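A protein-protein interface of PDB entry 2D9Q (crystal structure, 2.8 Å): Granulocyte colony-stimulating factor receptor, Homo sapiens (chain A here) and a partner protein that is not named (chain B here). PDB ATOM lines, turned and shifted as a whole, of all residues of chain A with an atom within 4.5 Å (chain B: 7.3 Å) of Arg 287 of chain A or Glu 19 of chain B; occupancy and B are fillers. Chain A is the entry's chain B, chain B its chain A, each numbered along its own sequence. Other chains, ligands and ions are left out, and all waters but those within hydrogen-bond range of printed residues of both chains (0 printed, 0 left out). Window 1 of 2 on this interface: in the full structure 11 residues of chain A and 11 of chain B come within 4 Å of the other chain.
The side-chain amide nitrogen (NE2) of Gln 20 of chain B sits close to the backbone NH (N) of Phe 113 of chain B, 3.0 Å away. The side-chain sulfur (SD) of Met 198 of chain A lies close to the side-chain hydroxyl (OH) of Tyr 172 of chain A (3.8 Å). NH1 of Arg 287 of chain A is in hydrogen-bond range of O of Met 198 of chain A, 3.1 Å away. OE1 of Gln 240 of chain A lies close to O of Ile 238 of chain A (3.1 Å). The backbone NH (N) of Trp 288 of chain A is in hydrogen-bond range of the backbone carbonyl oxygen (O) of Asn 239 of chain A (2.8 Å). The guanidinium group of Arg 287 of chain A lies within hydrogen-bond range of the backbone carbonyl oxygen of Pro 291 of chain A.
Printed residues of chain B within 4 Å of Arg 287 of chain A: Glu 19 (2.6 Å). Printed residues of chain A within 4 Å of Glu 19 of chain B: Tyr 172, His 237, Ile 238 and Arg 287. Printed residues of chain B within 4 Å of Asn 239 of chain A: Arg 22. Printed residues of chain B within 4 Å of His 237 of chain A: Glu 19 (3.4 Å), Arg 22 (3.4 Å) and Lys 23 (3.1 Å). Of the printed residues of chain B, Leu 290 of chain A touches Lys 16 (3.99 Å). The nearest residue of chain B that does not touch Arg 287 of chain A is Lys 16 of chain B (5.0 Å). The nearest printed residue of chain B that does not touch Leu 290 of chain A is Leu 15 of chain B (4.001 Å).
Tyr 172 of chain A touches Gln 20 of chain B. His 237 of chain A touches Glu 19 of chain B. CB of Lys 23 of chain B touches ND1 of His 237 of chain A, 3.1 Å away. Ile 238 of chain A touches Glu 19 of chain B (CG1 to OE2, 3.5 Å). Asn 239 of chain A touches Arg 22 of chain B (ND2 to CZ, 3.4 Å). CD2 of Leu 290 of chain A touches CG of Lys 16 of chain B (3.99 Å).
The guanidinium group (NH2) of Arg 287 of chain A is in salt-bridge range of the side-chain carboxylate (OE1) of Glu 19 of chain B (2.6 Å). NE of Arg 22 of chain B lies within hydrogen-bond range of O of His 237 of chain A, 3.4 Å away. The side-chain hydroxyl of Tyr 172 of chain A lies close to the side-chain carboxylate of Glu 19 of chain B, at 2.3 Å.
Of the 15 printed residues of chain A, 6 touch a printed residue of chain B. Hydrophobic or aromatic side chains of chain A within 4 Å of the printed part of chain B: Tyr 172, His 237, Ile 238 and Leu 290. Of the 15 printed residues of chain B, 5 touch a printed residue of chain A. Among the printed residues, 9 pairs touch across the chains. Among the printed residues, Asp or Glu carboxylates within 4 Å of a Lys or Arg side-chain nitrogen of the other chain: Arg 287 of chain A with Glu 19 of chain B (2.6 Å).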
ATOM      1  N   TYR A 172      -6.052 -22.409  -9.920  1.00  0.00           N
ATOM      2  CA  TYR A 172      -6.947 -22.900 -11.001  1.00  0.00           C
ATOM      3  C   TYR A 172      -7.902 -23.983 -10.555  1.00  0.00           C
ATOM      4  O   TYR A 172      -7.912 -25.034 -11.120  1.00  0.00           O
ATOM      5  CB  TYR A 172      -6.113 -23.435 -12.212  1.00  0.00           C
ATOM      6  CG  TYR A 172      -5.287 -22.340 -12.870  1.00  0.00           C
ATOM      7  CD1 TYR A 172      -5.872 -21.311 -13.639  1.00  0.00           C
ATOM      8  CD2 TYR A 172      -3.919 -22.245 -12.608  1.00  0.00           C
ATOM      9  CE1 TYR A 172      -5.065 -20.279 -14.157  1.00  0.00           C
ATOM     10  CE2 TYR A 172      -3.114 -21.195 -13.176  1.00  0.00           C
ATOM     11  CZ  TYR A 172      -3.684 -20.252 -13.932  1.00  0.00           C
ATOM     12  OH  TYR A 172      -2.829 -19.282 -14.387  1.00  0.00           O
ATOM     13  N   MET A 198      -7.000 -17.601  -8.769  1.00  0.00           N
ATOM     14  CA  MET A 198      -6.453 -17.032  -9.988  1.00  0.00           C
ATOM     15  C   MET A 198      -7.365 -15.963 -10.592  1.00  0.00           C
ATOM     16  O   MET A 198      -6.899 -15.123 -11.363  1.00  0.00           O
ATOM     17  CB  MET A 198      -6.143 -18.130 -10.965  1.00  0.00           C
ATOM     18  CG  MET A 198      -4.848 -17.949 -11.720  1.00  0.00           C
ATOM     19  SD  MET A 198      -3.383 -18.226 -10.808  1.00  0.00           S
ATOM     20  CE  MET A 198      -2.694 -16.419 -11.256  1.00  0.00           C
ATOM     21  N   ASP A 199      -8.634 -15.931 -10.191  1.00  0.00           N
ATOM     22  CA  ASP A 199      -9.516 -14.929 -10.742  1.00  0.00           C
ATOM     23  C   ASP A 199      -9.628 -13.766  -9.802  1.00  0.00           C
ATOM     24  O   ASP A 199     -10.478 -12.930  -9.970  1.00  0.00           O
ATOM     25  CB  ASP A 199     -10.930 -15.464 -10.949  1.00  0.00           C
ATOM     26  CG  ASP A 199     -11.002 -16.877 -11.620  1.00  0.00           C
ATOM     27  OD1 ASP A 199     -10.266 -17.342 -12.566  1.00  0.00           O
ATOM     28  OD2 ASP A 199     -11.899 -17.601 -11.197  1.00  0.00           O
ATOM     29  N   LEU A 203      -3.479  -7.268 -10.278  1.00  0.00           N
ATOM     30  CA  LEU A 203      -2.438  -6.775 -11.146  1.00  0.00           C
ATOM     31  C   LEU A 203      -1.891  -5.401 -10.833  1.00  0.00           C
ATOM     32  O   LEU A 203      -2.384  -4.635 -10.048  1.00  0.00           O
ATOM     33  CB  LEU A 203      -2.941  -6.766 -12.548  1.00  0.00           C
ATOM     34  CG  LEU A 203      -3.421  -8.103 -13.126  1.00  0.00           C
ATOM     35  CD1 LEU A 203      -4.302  -7.701 -14.314  1.00  0.00           C
ATOM     36  CD2 LEU A 203      -2.258  -9.090 -13.568  1.00  0.00           C
ATOM     37  N   HIS A 237       2.833 -13.286 -17.547  1.00  0.00           N
ATOM     38  CA  HIS A 237       2.457 -14.654 -17.895  1.00  0.00           C
ATOM     39  C   HIS A 237       0.939 -14.833 -18.057  1.00  0.00           C
ATOM     40  O   HIS A 237       0.459 -15.971 -17.984  1.00  0.00           O
ATOM     41  CB  HIS A 237       3.059 -15.637 -16.805  1.00  0.00           C
ATOM     42  CG  HIS A 237       2.333 -15.646 -15.492  1.00  0.00           C
ATOM     43  ND1 HIS A 237       1.890 -16.807 -14.896  1.00  0.00           N
ATOM     44  CD2 HIS A 237       1.913 -14.643 -14.690  1.00  0.00           C
ATOM     45  CE1 HIS A 237       1.195 -16.537 -13.793  1.00  0.00           C
ATOM     46  NE2 HIS A 237       1.192 -15.221 -13.648  1.00  0.00           N
ATOM     47  N   ILE A 238       0.194 -13.723 -18.218  1.00  0.00           N
ATOM     48  CA  ILE A 238      -1.268 -13.654 -18.031  1.00  0.00           C
ATOM     49  C   ILE A 238      -1.815 -12.726 -19.055  1.00  0.00           C
ATOM     50  O   ILE A 238      -1.569 -11.497 -18.939  1.00  0.00           O
ATOM     51  CB  ILE A 238      -1.605 -12.988 -16.730  1.00  0.00           C
ATOM     52  CG1 ILE A 238      -1.496 -13.939 -15.554  1.00  0.00           C
ATOM     53  CG2 ILE A 238      -2.985 -12.447 -16.760  1.00  0.00           C
ATOM     54  CD1 ILE A 238      -1.647 -13.215 -14.139  1.00  0.00           C
ATOM     55  N   ASN A 239      -2.586 -13.259 -20.017  1.00  0.00           N
ATOM     56  CA  ASN A 239      -2.974 -12.412 -21.194  1.00  0.00           C
ATOM     57  C   ASN A 239      -3.970 -11.443 -20.698  1.00  0.00           C
ATOM     58  O   ASN A 239      -5.071 -11.814 -20.327  1.00  0.00           O
ATOM     59  CB  ASN A 239      -3.524 -13.127 -22.496  1.00  0.00           C
ATOM     60  CG  ASN A 239      -2.635 -14.368 -22.997  1.00  0.00           C
ATOM     61  OD1 ASN A 239      -3.211 -15.244 -23.601  1.00  0.00           O
ATOM     62  ND2 ASN A 239      -1.270 -14.421 -22.754  1.00  0.00           N
ATOM     63  N   GLN A 240      -3.587 -10.200 -20.696  1.00  0.00           N
ATOM     64  CA  GLN A 240      -4.440  -9.270 -20.106  1.00  0.00           C
ATOM     65  C   GLN A 240      -4.850  -8.194 -21.120  1.00  0.00           C
ATOM     66  O   GLN A 240      -4.288  -8.101 -22.130  1.00  0.00           O
ATOM     67  CB  GLN A 240      -3.762  -8.779 -18.840  1.00  0.00           C
ATOM     68  CG  GLN A 240      -2.481  -8.028 -19.016  1.00  0.00           C
ATOM     69  CD  GLN A 240      -1.697  -7.913 -17.759  1.00  0.00           C
ATOM     70  OE1 GLN A 240      -1.120  -8.914 -17.317  1.00  0.00           O
ATOM     71  NE2 GLN A 240      -1.649  -6.690 -17.174  1.00  0.00           N
ATOM     72  N   ILE A 286      -6.100  -5.624 -17.108  1.00  0.00           N
ATOM     73  CA  ILE A 286      -6.963  -6.590 -16.483  1.00  0.00           C
ATOM     74  C   ILE A 286      -6.876  -7.827 -17.252  1.00  0.00           C
ATOM     75  O   ILE A 286      -6.854  -7.776 -18.470  1.00  0.00           O
ATOM     76  CB  ILE A 286      -8.358  -6.112 -16.610  1.00  0.00           C
ATOM     77  CG1 ILE A 286      -9.351  -7.117 -16.096  1.00  0.00           C
ATOM     78  CG2 ILE A 286      -8.724  -5.972 -18.021  1.00  0.00           C
ATOM     79  CD1 ILE A 286     -10.745  -6.535 -16.038  1.00  0.00           C
ATOM     80  N   ARG A 287      -6.893  -8.949 -16.560  1.00  0.00           N
ATOM     81  CA  ARG A 287      -6.678 -10.255 -17.183  1.00  0.00           C
ATOM     82  C   ARG A 287      -7.811 -10.523 -18.106  1.00  0.00           C
ATOM     83  O   ARG A 287      -8.923 -10.163 -17.774  1.00  0.00           O
ATOM     84  CB  ARG A 287      -6.664 -11.255 -16.058  1.00  0.00           C
ATOM     85  CG  ARG A 287      -6.264 -12.740 -16.344  1.00  0.00           C
ATOM     86  CD  ARG A 287      -6.833 -13.657 -15.319  1.00  0.00           C
ATOM     87  NE  ARG A 287      -6.345 -14.993 -15.483  1.00  0.00           N
ATOM     88  CZ  ARG A 287      -6.965 -16.031 -14.898  1.00  0.00           C
ATOM     89  NH1 ARG A 287      -8.062 -15.821 -14.137  1.00  0.00           N
ATOM     90  NH2 ARG A 287      -6.509 -17.264 -15.065  1.00  0.00           N
ATOM     91  N   TRP A 288      -7.566 -11.066 -19.298  1.00  0.00           N
ATOM     92  CA  TRP A 288      -8.591 -10.774 -20.290  1.00  0.00           C
ATOM     93  C   TRP A 288      -9.672 -11.794 -20.595  1.00  0.00           C
ATOM     94  O   TRP A 288     -10.818 -11.753 -20.034  1.00  0.00           O
ATOM     95  CB  TRP A 288      -8.215 -10.018 -21.550  1.00  0.00           C
ATOM     96  CG  TRP A 288      -9.550  -9.654 -22.218  1.00  0.00           C
ATOM     97  CD1 TRP A 288     -10.683  -9.139 -21.623  1.00  0.00           C
ATOM     98  CD2 TRP A 288      -9.891  -9.925 -23.546  1.00  0.00           C
ATOM     99  NE1 TRP A 288     -11.703  -9.068 -22.525  1.00  0.00           N
ATOM    100  CE2 TRP A 288     -11.226  -9.532 -23.732  1.00  0.00           C
ATOM    101  CE3 TRP A 288      -9.174 -10.441 -24.652  1.00  0.00           C
ATOM    102  CZ2 TRP A 288     -11.879  -9.643 -25.035  1.00  0.00           C
ATOM    103  CZ3 TRP A 288      -9.795 -10.577 -25.919  1.00  0.00           C
ATOM    104  CH2 TRP A 288     -11.137 -10.176 -26.111  1.00  0.00           C
ATOM    105  N   PRO A 289      -9.432 -12.725 -21.450  1.00  0.00           N
ATOM    106  CA  PRO A 289     -10.580 -13.640 -21.703  1.00  0.00           C
ATOM    107  C   PRO A 289     -10.981 -14.388 -20.296  1.00  0.00           C
ATOM    108  O   PRO A 289     -12.151 -14.591 -19.824  1.00  0.00           O
ATOM    109  CB  PRO A 289     -10.082 -14.495 -22.828  1.00  0.00           C
ATOM    110  CG  PRO A 289      -8.853 -13.662 -23.290  1.00  0.00           C
ATOM    111  CD  PRO A 289      -8.131 -13.090 -22.026  1.00  0.00           C
ATOM    112  N   LEU A 290      -9.939 -14.650 -19.522  1.00  0.00           N
ATOM    113  CA  LEU A 290     -10.168 -15.146 -18.209  1.00  0.00           C
ATOM    114  C   LEU A 290     -10.638 -14.048 -17.252  1.00  0.00           C
ATOM    115  O   LEU A 290     -10.384 -12.861 -17.420  1.00  0.00           O
ATOM    116  CB  LEU A 290      -8.890 -15.879 -17.727  1.00  0.00           C
ATOM    117  CG  LEU A 290      -8.531 -17.089 -18.609  1.00  0.00           C
ATOM    118  CD1 LEU A 290      -7.278 -17.690 -18.276  1.00  0.00           C
ATOM    119  CD2 LEU A 290      -9.636 -18.186 -18.577  1.00  0.00           C
ATOM    120  N   PRO A 291     -11.246 -14.501 -16.178  1.00  0.00           N
ATOM    121  CA  PRO A 291     -11.751 -13.605 -15.181  1.00  0.00           C
ATOM    122  C   PRO A 291     -10.618 -12.838 -14.451  1.00  0.00           C
ATOM    123  O   PRO A 291      -9.496 -13.351 -14.139  1.00  0.00           O
ATOM    124  CB  PRO A 291     -12.413 -14.577 -14.201  1.00  0.00           C
ATOM    125  CG  PRO A 291     -12.366 -15.953 -14.799  1.00  0.00           C
ATOM    126  CD  PRO A 291     -11.335 -15.922 -15.786  1.00  0.00           C
ATOM    127  N   GLY A 292     -10.915 -11.607 -14.108  1.00  0.00           N
ATOM    128  CA  GLY A 292      -9.954 -10.868 -13.314  1.00  0.00           C
ATOM    129  C   GLY A 292     -10.476  -9.500 -13.026  1.00  0.00           C
ATOM    130  O   GLY A 292     -11.469  -9.195 -13.585  1.00  0.00           O
ATOM    131  N   LEU B  14      -8.810 -24.198 -21.936  1.00  0.00           N
ATOM    132  CA  LEU B  14      -7.616 -24.214 -22.739  1.00  0.00           C
ATOM    133  C   LEU B  14      -6.753 -23.067 -22.418  1.00  0.00           C
ATOM    134  O   LEU B  14      -5.541 -23.211 -22.451  1.00  0.00           O
ATOM    135  CB  LEU B  14      -7.953 -24.069 -24.218  1.00  0.00           C
ATOM    136  CG  LEU B  14      -8.319 -25.297 -25.053  1.00  0.00           C
ATOM    137  CD1 LEU B  14      -8.022 -24.833 -26.470  1.00  0.00           C
ATOM    138  CD2 LEU B  14      -7.615 -26.624 -24.741  1.00  0.00           C
ATOM    139  N   LEU B  15      -7.376 -21.906 -22.243  1.00  0.00           N
ATOM    140  CA  LEU B  15      -6.619 -20.723 -21.944  1.00  0.00           C
ATOM    141  C   LEU B  15      -6.054 -20.835 -20.557  1.00  0.00           C
ATOM    142  O   LEU B  15      -4.990 -20.282 -20.289  1.00  0.00           O
ATOM    143  CB  LEU B  15      -7.497 -19.538 -21.853  1.00  0.00           C
ATOM    144  CG  LEU B  15      -7.935 -18.974 -23.137  1.00  0.00           C
ATOM    145  CD1 LEU B  15      -9.407 -18.831 -22.891  1.00  0.00           C
ATOM    146  CD2 LEU B  15      -7.225 -17.639 -23.205  1.00  0.00           C
ATOM    147  N   LYS B  16      -6.794 -21.451 -19.643  1.00  0.00           N
ATOM    148  CA  LYS B  16      -6.218 -21.673 -18.362  1.00  0.00           C
ATOM    149  C   LYS B  16      -4.992 -22.556 -18.531  1.00  0.00           C
ATOM    150  O   LYS B  16      -4.159 -22.575 -17.660  1.00  0.00           O
ATOM    151  CB  LYS B  16      -7.164 -22.358 -17.405  1.00  0.00           C
ATOM    152  CG  LYS B  16      -8.374 -21.547 -16.841  1.00  0.00           C
ATOM    153  CD  LYS B  16      -9.426 -22.545 -16.228  1.00  0.00           C
ATOM    154  CE  LYS B  16     -10.371 -22.017 -15.134  1.00  0.00           C
ATOM    155  NZ  LYS B  16     -11.351 -20.972 -15.589  1.00  0.00           N
ATOM    156  N   CYS B  17      -4.856 -23.312 -19.604  1.00  0.00           N
ATOM    157  CA  CYS B  17      -3.796 -24.314 -19.654  1.00  0.00           C
ATOM    158  C   CYS B  17      -2.581 -23.656 -20.137  1.00  0.00           C
ATOM    159  O   CYS B  17      -1.446 -24.083 -19.863  1.00  0.00           O
ATOM    160  CB  CYS B  17      -4.102 -25.406 -20.637  1.00  0.00           C
ATOM    161  SG  CYS B  17      -4.882 -26.830 -19.939  1.00  0.00           S
ATOM    162  N   LEU B  18      -2.815 -22.603 -20.882  1.00  0.00           N
ATOM    163  CA  LEU B  18      -1.741 -21.923 -21.576  1.00  0.00           C
ATOM    164  C   LEU B  18      -1.093 -20.993 -20.588  1.00  0.00           C
ATOM    165  O   LEU B  18       0.109 -20.821 -20.578  1.00  0.00           O
ATOM    166  CB  LEU B  18      -2.312 -21.097 -22.736  1.00  0.00           C
ATOM    167  CG  LEU B  18      -2.007 -21.457 -24.204  1.00  0.00           C
ATOM    168  CD1 LEU B  18      -2.233 -22.993 -24.471  1.00  0.00           C
ATOM    169  CD2 LEU B  18      -2.896 -20.524 -25.125  1.00  0.00           C
ATOM    170  N   GLU B  19      -1.912 -20.376 -19.757  1.00  0.00           N
ATOM    171  CA  GLU B  19      -1.390 -19.567 -18.699  1.00  0.00           C
ATOM    172  C   GLU B  19      -0.416 -20.362 -17.958  1.00  0.00           C
ATOM    173  O   GLU B  19       0.710 -19.930 -17.786  1.00  0.00           O
ATOM    174  CB  GLU B  19      -2.474 -19.198 -17.716  1.00  0.00           C
ATOM    175  CG  GLU B  19      -2.289 -17.758 -17.191  1.00  0.00           C
ATOM    176  CD  GLU B  19      -3.521 -17.200 -16.519  1.00  0.00           C
ATOM    177  OE1 GLU B  19      -4.075 -17.896 -15.649  1.00  0.00           O
ATOM    178  OE2 GLU B  19      -3.888 -16.065 -16.897  1.00  0.00           O
ATOM    179  N   GLN B  20      -0.851 -21.514 -17.495  1.00  0.00           N
ATOM    180  CA  GLN B  20      -0.032 -22.315 -16.645  1.00  0.00           C
ATOM    181  C   GLN B  20       1.231 -22.683 -17.351  1.00  0.00           C
ATOM    182  O   GLN B  20       2.385 -22.833 -16.758  1.00  0.00           O
ATOM    183  CB  GLN B  20      -0.767 -23.558 -16.263  1.00  0.00           C
ATOM    184  CG  GLN B  20      -2.050 -23.230 -15.613  1.00  0.00           C
ATOM    185  CD  GLN B  20      -2.544 -24.365 -14.746  1.00  0.00           C
ATOM    186  OE1 GLN B  20      -3.728 -24.463 -14.521  1.00  0.00           O
ATOM    187  NE2 GLN B  20      -1.639 -25.182 -14.190  1.00  0.00           N
ATOM    188  N   VAL B  21       1.092 -22.892 -18.639  1.00  0.00           N
ATOM    189  CA  VAL B  21       2.359 -23.214 -19.315  1.00  0.00           C
ATOM    190  C   VAL B  21       3.293 -22.025 -19.161  1.00  0.00           C
ATOM    191  O   VAL B  21       4.312 -22.190 -18.418  1.00  0.00           O
ATOM    192  CB  VAL B  21       2.190 -23.691 -20.715  1.00  0.00           C
ATOM    193  CG1 VAL B  21       3.479 -23.850 -21.356  1.00  0.00           C
ATOM    194  CG2 VAL B  21       1.573 -25.009 -20.617  1.00  0.00           C
ATOM    195  N   ARG B  22       2.931 -20.861 -19.760  1.00  0.00           N
ATOM    196  CA  ARG B  22       3.798 -19.692 -19.699  1.00  0.00           C
ATOM    197  C   ARG B  22       4.337 -19.609 -18.284  1.00  0.00           C
ATOM    198  O   ARG B  22       5.493 -19.266 -18.064  1.00  0.00           O
ATOM    199  CB  ARG B  22       3.115 -18.397 -20.048  1.00  0.00           C
ATOM    200  CG  ARG B  22       2.921 -18.238 -21.519  1.00  0.00           C
ATOM    201  CD  ARG B  22       1.915 -17.150 -22.077  1.00  0.00           C
ATOM    202  NE  ARG B  22       0.676 -17.024 -21.235  1.00  0.00           N
ATOM    203  CZ  ARG B  22      -0.552 -17.509 -21.524  1.00  0.00           C
ATOM    204  NH1 ARG B  22      -0.745 -18.136 -22.680  1.00  0.00           N
ATOM    205  NH2 ARG B  22      -1.582 -17.313 -20.686  1.00  0.00           N
ATOM    206  N   LYS B  23       3.520 -19.944 -17.297  1.00  0.00           N
ATOM    207  CA  LYS B  23       3.989 -19.754 -15.933  1.00  0.00           C
ATOM    208  C   LYS B  23       5.107 -20.749 -15.578  1.00  0.00           C
ATOM    209  O   LYS B  23       6.202 -20.333 -15.225  1.00  0.00           O
ATOM    210  CB  LYS B  23       2.814 -19.802 -14.909  1.00  0.00           C
ATOM    211  CG  LYS B  23       3.262 -19.951 -13.343  1.00  0.00           C
ATOM    212  CD  LYS B  23       4.091 -18.649 -12.775  1.00  0.00           C
ATOM    213  CE  LYS B  23       4.527 -18.798 -11.354  1.00  0.00           C
ATOM    214  NZ  LYS B  23       3.470 -19.481 -10.519  1.00  0.00           N
ATOM    215  N   ILE B  24       4.818 -22.039 -15.670  1.00  0.00           N
ATOM    216  CA  ILE B  24       5.824 -23.001 -15.478  1.00  0.00           C
ATOM    217  C   ILE B  24       7.046 -22.725 -16.338  1.00  0.00           C
ATOM    218  O   ILE B  24       8.127 -23.075 -15.992  1.00  0.00           O
ATOM    219  CB  ILE B  24       5.306 -24.331 -15.849  1.00  0.00           C
ATOM    220  CG1 ILE B  24       4.007 -24.618 -15.099  1.00  0.00           C
ATOM    221  CG2 ILE B  24       6.396 -25.327 -15.547  1.00  0.00           C
ATOM    222  CD1 ILE B  24       3.624 -26.101 -15.024  1.00  0.00           C
ATOM    223  N   GLN B  25       6.909 -22.148 -17.512  1.00  0.00           N
ATOM    224  CA  GLN B  25       8.138 -21.926 -18.361  1.00  0.00           C
ATOM    225  C   GLN B  25       9.081 -21.030 -17.613  1.00  0.00           C
ATOM    226  O   GLN B  25      10.228 -21.358 -17.372  1.00  0.00           O
ATOM    227  CB  GLN B  25       7.814 -21.292 -19.725  1.00  0.00           C
ATOM    228  CG  GLN B  25       6.976 -22.293 -20.613  1.00  0.00           C
ATOM    229  CD  GLN B  25       7.025 -22.027 -22.162  1.00  0.00           C
ATOM    230  OE1 GLN B  25       6.233 -21.195 -22.742  1.00  0.00           O
ATOM    231  NE2 GLN B  25       7.964 -22.748 -22.835  1.00  0.00           N
ATOM    232  N   PHE B 113      -0.975 -27.851 -12.960  1.00  0.00           N
ATOM    233  CA  PHE B 113      -1.257 -28.005 -14.381  1.00  0.00           C
ATOM    234  C   PHE B 113      -1.592 -29.402 -14.572  1.00  0.00           C
ATOM    235  O   PHE B 113      -2.392 -29.766 -15.372  1.00  0.00           O
ATOM    236  CB  PHE B 113       0.007 -27.836 -15.164  1.00  0.00           C
ATOM    237  CG  PHE B 113      -0.185 -27.697 -16.643  1.00  0.00           C
ATOM    238  CD1 PHE B 113      -1.349 -27.222 -17.158  1.00  0.00           C
ATOM    239  CD2 PHE B 113       0.842 -27.992 -17.494  1.00  0.00           C
ATOM    240  CE1 PHE B 113      -1.480 -27.066 -18.433  1.00  0.00           C
ATOM    241  CE2 PHE B 113       0.694 -27.858 -18.743  1.00  0.00           C
ATOM    242  CZ  PHE B 113      -0.464 -27.382 -19.227  1.00  0.00           C
ATOM    243  N   TYR B 165       2.737 -26.410 -25.623  1.00  0.00           N
ATOM    244  CA  TYR B 165       2.195 -25.154 -26.075  1.00  0.00           C
ATOM    245  C   TYR B 165       1.531 -25.285 -27.348  1.00  0.00           C
ATOM    246  O   TYR B 165       0.399 -24.956 -27.412  1.00  0.00           O
ATOM    247  CB  TYR B 165       3.184 -24.090 -26.347  1.00  0.00           C
ATOM    248  CG  TYR B 165       2.617 -22.739 -26.090  1.00  0.00           C
ATOM    249  CD1 TYR B 165       2.315 -22.328 -24.772  1.00  0.00           C
ATOM    250  CD2 TYR B 165       2.381 -21.853 -27.148  1.00  0.00           C
ATOM    251  CE1 TYR B 165       1.786 -21.055 -24.503  1.00  0.00           C
ATOM    252  CE2 TYR B 165       1.850 -20.513 -26.900  1.00  0.00           C
ATOM    253  CZ  TYR B 165       1.546 -20.121 -25.569  1.00  0.00           C
ATOM    254  OH  TYR B 165       1.025 -18.846 -25.307  1.00  0.00           O
ATOM    255  N   LEU B 168      -1.714 -26.746 -28.006  1.00  0.00           N
ATOM    256  CA  LEU B 168      -2.835 -26.179 -27.308  1.00  0.00           C
ATOM    257  C   LEU B 168      -3.156 -24.981 -28.056  1.00  0.00           C
ATOM    258  O   LEU B 168      -4.264 -24.733 -28.190  1.00  0.00           O
ATOM    259  CB  LEU B 168      -2.547 -25.822 -25.846  1.00  0.00           C
ATOM    260  CG  LEU B 168      -2.346 -26.983 -24.821  1.00  0.00           C
ATOM    261  CD1 LEU B 168      -1.787 -26.557 -23.391  1.00  0.00           C
ATOM    262  CD2 LEU B 168      -3.575 -27.909 -24.615  1.00  0.00           C
